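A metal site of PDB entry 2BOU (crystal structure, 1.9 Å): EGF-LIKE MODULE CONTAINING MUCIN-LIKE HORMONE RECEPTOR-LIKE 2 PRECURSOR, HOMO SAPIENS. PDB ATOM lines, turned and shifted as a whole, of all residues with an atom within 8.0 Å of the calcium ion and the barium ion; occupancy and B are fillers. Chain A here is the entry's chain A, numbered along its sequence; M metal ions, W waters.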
ATOM      1  N   PRO A  25      -5.044   1.480  -1.999  1.00  0.00           N
ATOM      2  CA  PRO A  25      -4.102   1.500  -0.879  1.00  0.00           C
ATOM      3  C   PRO A  25      -2.681   1.273  -1.371  1.00  0.00           C
ATOM      4  O   PRO A  25      -2.430   0.408  -2.201  1.00  0.00           O
ATOM      5  CB  PRO A  25      -4.562   0.313  -0.028  1.00  0.00           C
ATOM      6  CG  PRO A  25      -6.042   0.230  -0.269  1.00  0.00           C
ATOM      7  CD  PRO A  25      -6.275   0.745  -1.678  1.00  0.00           C
ATOM      8  N   GLY A  26      -1.747   2.063  -0.864  1.00  0.00           N
ATOM      9  CA  GLY A  26      -0.351   1.930  -1.247  1.00  0.00           C
ATOM     10  C   GLY A  26       0.043   2.850  -2.400  1.00  0.00           C
ATOM     11  O   GLY A  26       1.186   2.838  -2.835  1.00  0.00           O
ATOM     12  N   PHE A  27      -0.900   3.630  -2.899  1.00  0.00           N
ATOM     13  CA  PHE A  27      -0.627   4.577  -3.983  1.00  0.00           C
ATOM     14  C   PHE A  27      -1.092   5.957  -3.564  1.00  0.00           C
ATOM     15  O   PHE A  27      -1.948   6.103  -2.703  1.00  0.00           O
ATOM     16  CB  PHE A  27      -1.338   4.165  -5.276  1.00  0.00           C
ATOM     17  CG  PHE A  27      -0.900   2.832  -5.816  1.00  0.00           C
ATOM     18  CD1 PHE A  27      -1.496   1.659  -5.370  1.00  0.00           C
ATOM     19  CD2 PHE A  27       0.125   2.753  -6.735  1.00  0.00           C
ATOM     20  CE1 PHE A  27      -1.092   0.428  -5.864  1.00  0.00           C
ATOM     21  CE2 PHE A  27       0.525   1.517  -7.249  1.00  0.00           C
ATOM     22  CZ  PHE A  27      -0.079   0.363  -6.806  1.00  0.00           C
ATOM     23  N   ASP A  42       0.658   7.144  -7.876  1.00  0.00           N
ATOM     24  CA  ASP A  42       2.023   6.654  -7.827  1.00  0.00           C
ATOM     25  C   ASP A  42       2.275   5.780  -6.610  1.00  0.00           C
ATOM     26  O   ASP A  42       1.757   6.039  -5.526  1.00  0.00           O
ATOM     27  CB  ASP A  42       2.993   7.825  -7.822  1.00  0.00           C
ATOM     28  CG  ASP A  42       2.798   8.734  -9.027  1.00  0.00           C
ATOM     29  OD1 ASP A  42       2.544   8.205 -10.119  1.00  0.00           O
ATOM     30  OD2 ASP A  42       2.842   9.972  -8.849  1.00  0.00           O
ATOM     31  N   ASP A  43       3.081   4.732  -6.795  1.00  0.00           N
ATOM     32  CA  ASP A  43       3.395   3.843  -5.691  1.00  0.00           C
ATOM     33  C   ASP A  43       4.044   4.618  -4.563  1.00  0.00           C
ATOM     34  O   ASP A  43       4.854   5.507  -4.787  1.00  0.00           O
ATOM     35  CB  ASP A  43       4.325   2.705  -6.141  1.00  0.00           C
ATOM     36  CG  ASP A  43       4.738   1.799  -4.978  1.00  0.00           C
ATOM     37  OD1 ASP A  43       3.845   1.165  -4.370  1.00  0.00           O
ATOM     38  OD2 ASP A  43       5.923   1.832  -4.597  1.00  0.00           O
ATOM     39  N   ILE A  44       3.654   4.276  -3.335  1.00  0.00           N
ATOM     40  CA  ILE A  44       4.260   4.888  -2.172  1.00  0.00           C
ATOM     41  C   ILE A  44       5.406   3.984  -1.725  1.00  0.00           C
ATOM     42  O   ILE A  44       5.215   2.779  -1.600  1.00  0.00           O
ATOM     43  CB  ILE A  44       3.259   4.991  -1.013  1.00  0.00           C
ATOM     44  CG1 ILE A  44       2.194   6.058  -1.314  1.00  0.00           C
ATOM     45  CG2 ILE A  44       3.980   5.290   0.294  1.00  0.00           C
ATOM     46  CD1 ILE A  44       0.841   5.764  -0.716  1.00  0.00           C
ATOM     47  N   ASN A  45       6.587   4.539  -1.536  1.00  0.00           N
ATOM     48  CA  ASN A  45       7.709   3.732  -1.096  1.00  0.00           C
ATOM     49  C   ASN A  45       7.728   3.672   0.428  1.00  0.00           C
ATOM     50  O   ASN A  45       8.324   4.517   1.090  1.00  0.00           O
ATOM     51  CB  ASN A  45       9.041   4.269  -1.620  1.00  0.00           C
ATOM     52  CG  ASN A  45      10.232   3.425  -1.175  1.00  0.00           C
ATOM     53  OD1 ASN A  45      10.080   2.475  -0.416  1.00  0.00           O
ATOM     54  ND2 ASN A  45      11.421   3.796  -1.634  1.00  0.00           N
ATOM     55  N   GLU A  46       7.059   2.661   0.976  1.00  0.00           N
ATOM     56  CA  GLU A  46       6.997   2.492   2.425  1.00  0.00           C
ATOM     57  C   GLU A  46       8.377   2.393   3.070  1.00  0.00           C
ATOM     58  O   GLU A  46       8.541   2.767   4.237  1.00  0.00           O
ATOM     59  CB  GLU A  46       6.167   1.270   2.791  1.00  0.00           C
ATOM     60  CG  GLU A  46       4.669   1.443   2.569  1.00  0.00           C
ATOM     61  CD  GLU A  46       4.238   1.026   1.171  1.00  0.00           C
ATOM     62  OE1 GLU A  46       5.117   0.722   0.352  1.00  0.00           O
ATOM     63  OE2 GLU A  46       3.016   0.996   0.900  1.00  0.00           O
ATOM     64  N   CYS A  47       9.362   1.903   2.326  1.00  0.00           N
ATOM     65  CA  CYS A  47      10.705   1.723   2.893  1.00  0.00           C
ATOM     66  C   CYS A  47      11.479   3.023   3.104  1.00  0.00           C
ATOM     67  O   CYS A  47      12.534   3.021   3.727  1.00  0.00           O
ATOM     68  CB  CYS A  47      11.519   0.739   2.055  1.00  0.00           C
ATOM     69  SG  CYS A  47      10.750  -0.902   1.869  1.00  0.00           S
ATOM     70  N   TRP A  62      11.979  -4.145   1.428  1.00  0.00           N
ATOM     71  CA  TRP A  62      11.966  -4.148  -0.030  1.00  0.00           C
ATOM     72  C   TRP A  62      10.639  -3.583  -0.532  1.00  0.00           C
ATOM     73  O   TRP A  62       9.582  -4.125  -0.247  1.00  0.00           O
ATOM     74  CB  TRP A  62      12.168  -5.564  -0.579  1.00  0.00           C
ATOM     75  CG  TRP A  62      13.571  -6.068  -0.367  1.00  0.00           C
ATOM     76  CD1 TRP A  62      14.086  -6.590   0.782  1.00  0.00           C
ATOM     77  CD2 TRP A  62      14.625  -6.077  -1.328  1.00  0.00           C
ATOM     78  NE1 TRP A  62      15.404  -6.952   0.581  1.00  0.00           N
ATOM     79  CE2 TRP A  62      15.757  -6.645  -0.705  1.00  0.00           C
ATOM     80  CE3 TRP A  62      14.738  -5.655  -2.668  1.00  0.00           C
ATOM     81  CZ2 TRP A  62      16.985  -6.787  -1.356  1.00  0.00           C
ATOM     82  CZ3 TRP A  62      15.951  -5.812  -3.313  1.00  0.00           C
ATOM     83  CH2 TRP A  62      17.058  -6.374  -2.655  1.00  0.00           C
ATOM     84  N   ASN A  63      10.702  -2.464  -1.239  1.00  0.00           N
ATOM     85  CA  ASN A  63       9.492  -1.813  -1.762  1.00  0.00           C
ATOM     86  C   ASN A  63       8.935  -2.564  -2.965  1.00  0.00           C
ATOM     87  O   ASN A  63       9.690  -3.079  -3.785  1.00  0.00           O
ATOM     88  CB  ASN A  63       9.805  -0.359  -2.124  1.00  0.00           C
ATOM     89  CG  ASN A  63       8.583   0.391  -2.605  1.00  0.00           C
ATOM     90  OD1 ASN A  63       7.508   0.276  -2.039  1.00  0.00           O
ATOM     91  ND2 ASN A  63       8.754   1.185  -3.655  1.00  0.00           N
ATOM     92  N   THR A  64       7.612  -2.658  -3.045  1.00  0.00           N
ATOM     93  CA  THR A  64       6.917  -3.300  -4.174  1.00  0.00           C
ATOM     94  C   THR A  64       5.782  -2.384  -4.646  1.00  0.00           C
ATOM     95  O   THR A  64       5.513  -1.352  -4.028  1.00  0.00           O
ATOM     96  CB  THR A  64       6.316  -4.688  -3.782  1.00  0.00           C
ATOM     97  OG1 THR A  64       5.166  -4.496  -2.938  1.00  0.00           O
ATOM     98  CG2 THR A  64       7.331  -5.556  -3.047  1.00  0.00           C
ATOM     99  N   GLU A  65       5.110  -2.770  -5.724  1.00  0.00           N
ATOM    100  CA  GLU A  65       3.999  -1.973  -6.257  1.00  0.00           C
ATOM    101  C   GLU A  65       2.759  -2.219  -5.421  1.00  0.00           C
ATOM    102  O   GLU A  65       2.216  -3.319  -5.409  1.00  0.00           O
ATOM    103  CB  GLU A  65       3.707  -2.334  -7.715  1.00  0.00           C
ATOM    104  CG  GLU A  65       4.610  -1.661  -8.721  1.00  0.00           C
ATOM    105  CD  GLU A  65       4.507  -0.144  -8.684  1.00  0.00           C
ATOM    106  OE1 GLU A  65       5.529   0.512  -8.425  1.00  0.00           O
ATOM    107  OE2 GLU A  65       3.415   0.383  -8.972  1.00  0.00           O
ATOM    108  N   GLY A  66       2.319  -1.205  -4.692  1.00  0.00           N
ATOM    109  CA  GLY A  66       1.126  -1.335  -3.860  1.00  0.00           C
ATOM    110  C   GLY A  66       1.440  -1.863  -2.453  1.00  0.00           C
ATOM    111  O   GLY A  66       0.584  -1.868  -1.588  1.00  0.00           O
ATOM    112  N   SER A  67       2.687  -2.285  -2.229  1.00  0.00           N
ATOM    113  CA  SER A  67       3.068  -2.788  -0.903  1.00  0.00           C
ATOM    114  C   SER A  67       4.573  -2.723  -0.632  1.00  0.00           C
ATOM    115  O   SER A  67       5.292  -1.874  -1.163  1.00  0.00           O
ATOM    116  CB  SER A  67       2.547  -4.220  -0.715  1.00  0.00           C
ATOM    117  OG  SER A  67       2.337  -4.524   0.658  1.00  0.00           O
ATOM    118  N   TYR A  68       5.033  -3.625   0.228  1.00  0.00           N
ATOM    119  CA  TYR A  68       6.444  -3.724   0.586  1.00  0.00           C
ATOM    120  C   TYR A  68       6.571  -4.976   1.423  1.00  0.00           C
ATOM    121  O   TYR A  68       5.575  -5.521   1.885  1.00  0.00           O
ATOM    122  CB  TYR A  68       6.907  -2.507   1.397  1.00  0.00           C
ATOM    123  CG  TYR A  68       6.375  -2.485   2.809  1.00  0.00           C
ATOM    124  CD1 TYR A  68       7.104  -3.036   3.860  1.00  0.00           C
ATOM    125  CD2 TYR A  68       5.109  -1.960   3.087  1.00  0.00           C
ATOM    126  CE1 TYR A  68       6.607  -3.052   5.149  1.00  0.00           C
ATOM    127  CE2 TYR A  68       4.596  -1.961   4.376  1.00  0.00           C
ATOM    128  CZ  TYR A  68       5.352  -2.516   5.402  1.00  0.00           C
ATOM    129  OH  TYR A  68       4.849  -2.525   6.680  1.00  0.00           O
ATOM    130  N   ASP A  69       7.794  -5.459   1.602  1.00  0.00           N
ATOM    131  CA  ASP A  69       8.031  -6.640   2.412  1.00  0.00           C
ATOM    132  C   ASP A  69       9.297  -6.443   3.220  1.00  0.00           C
ATOM    133  O   ASP A  69      10.299  -5.973   2.681  1.00  0.00           O
ATOM    134  CB  ASP A  69       8.234  -7.879   1.530  1.00  0.00           C
ATOM    135  CG  ASP A  69       6.970  -8.319   0.819  1.00  0.00           C
ATOM    136  OD1 ASP A  69       6.044  -8.771   1.497  1.00  0.00           O
ATOM    137  OD2 ASP A  69       6.958  -8.310  -0.423  1.00  0.00           O
HETATM  138 CA    CA M   1       5.130   0.681  -2.188  1.00  0.00          CA
HETATM  139 BA    BA M   2       4.934  -0.061  -2.492  1.00  0.00          BA
HETATM  140  O   HOH W   1       2.860   0.971  -1.600  1.00  0.00           O
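OG1 of Thr 64 lies close to O of Ser 67. The side-chain hydroxyl (OG1) of Thr 64 is in hydrogen-bond range of the backbone NH (N) of Tyr 68 (3.3 Å). The backbone carbonyl oxygen (O) of Gly 26 sits at hydrogen-bond distance from the backbone NH (N) of Ile 44, at 2.9 Å. SG of Cys 47 sits at hydrogen-bond distance from N of Asn 63 (3.5 Å). OD1 of Asp 43 lies close to N of Gly 66 (2.8 Å).
Of the 17 residues printed, 6 come within 4 Å of the calcium ion.
Gly 66 touches the barium ion. Within 4 Å of the barium ion: Asp 43, Ile 44, Glu 46, Asn 63, Thr 64, Gly 66 and Ser 67.
The calcium ion is bound by the backbone carbonyl oxygen (O) of Ile 44 (2.2 Å), water W1 (2.4 Å), the side-chain amide oxygen (OD1) of Asn 63 (2.4 Å), the side-chain carboxylate (OE1) of Glu 46 (2.5 Å), the side-chain carboxylate (OD1) of Asp 43 (2.6 Å), the backbone carbonyl oxygen (O) of Ser 67 (2.8 Å), the backbone carbonyl oxygen (O) of Thr 64 (2.8 Å) and the side-chain carboxylate (OD2) of Asp 43 (2.8 Å).
The barium ion is bound by O of Thr 64, O of Ser 67, water W1, OD1 of Asp 43, OD1 of Asn 63, OE1 of Glu 46, O of Ile 44, OD2 of Asp 43 and N of Ser 67.
Water W1 lies within hydrogen-bond range of OE2 of Glu 46 (2.5 Å) and O of Gly 26 (2.8 Å).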
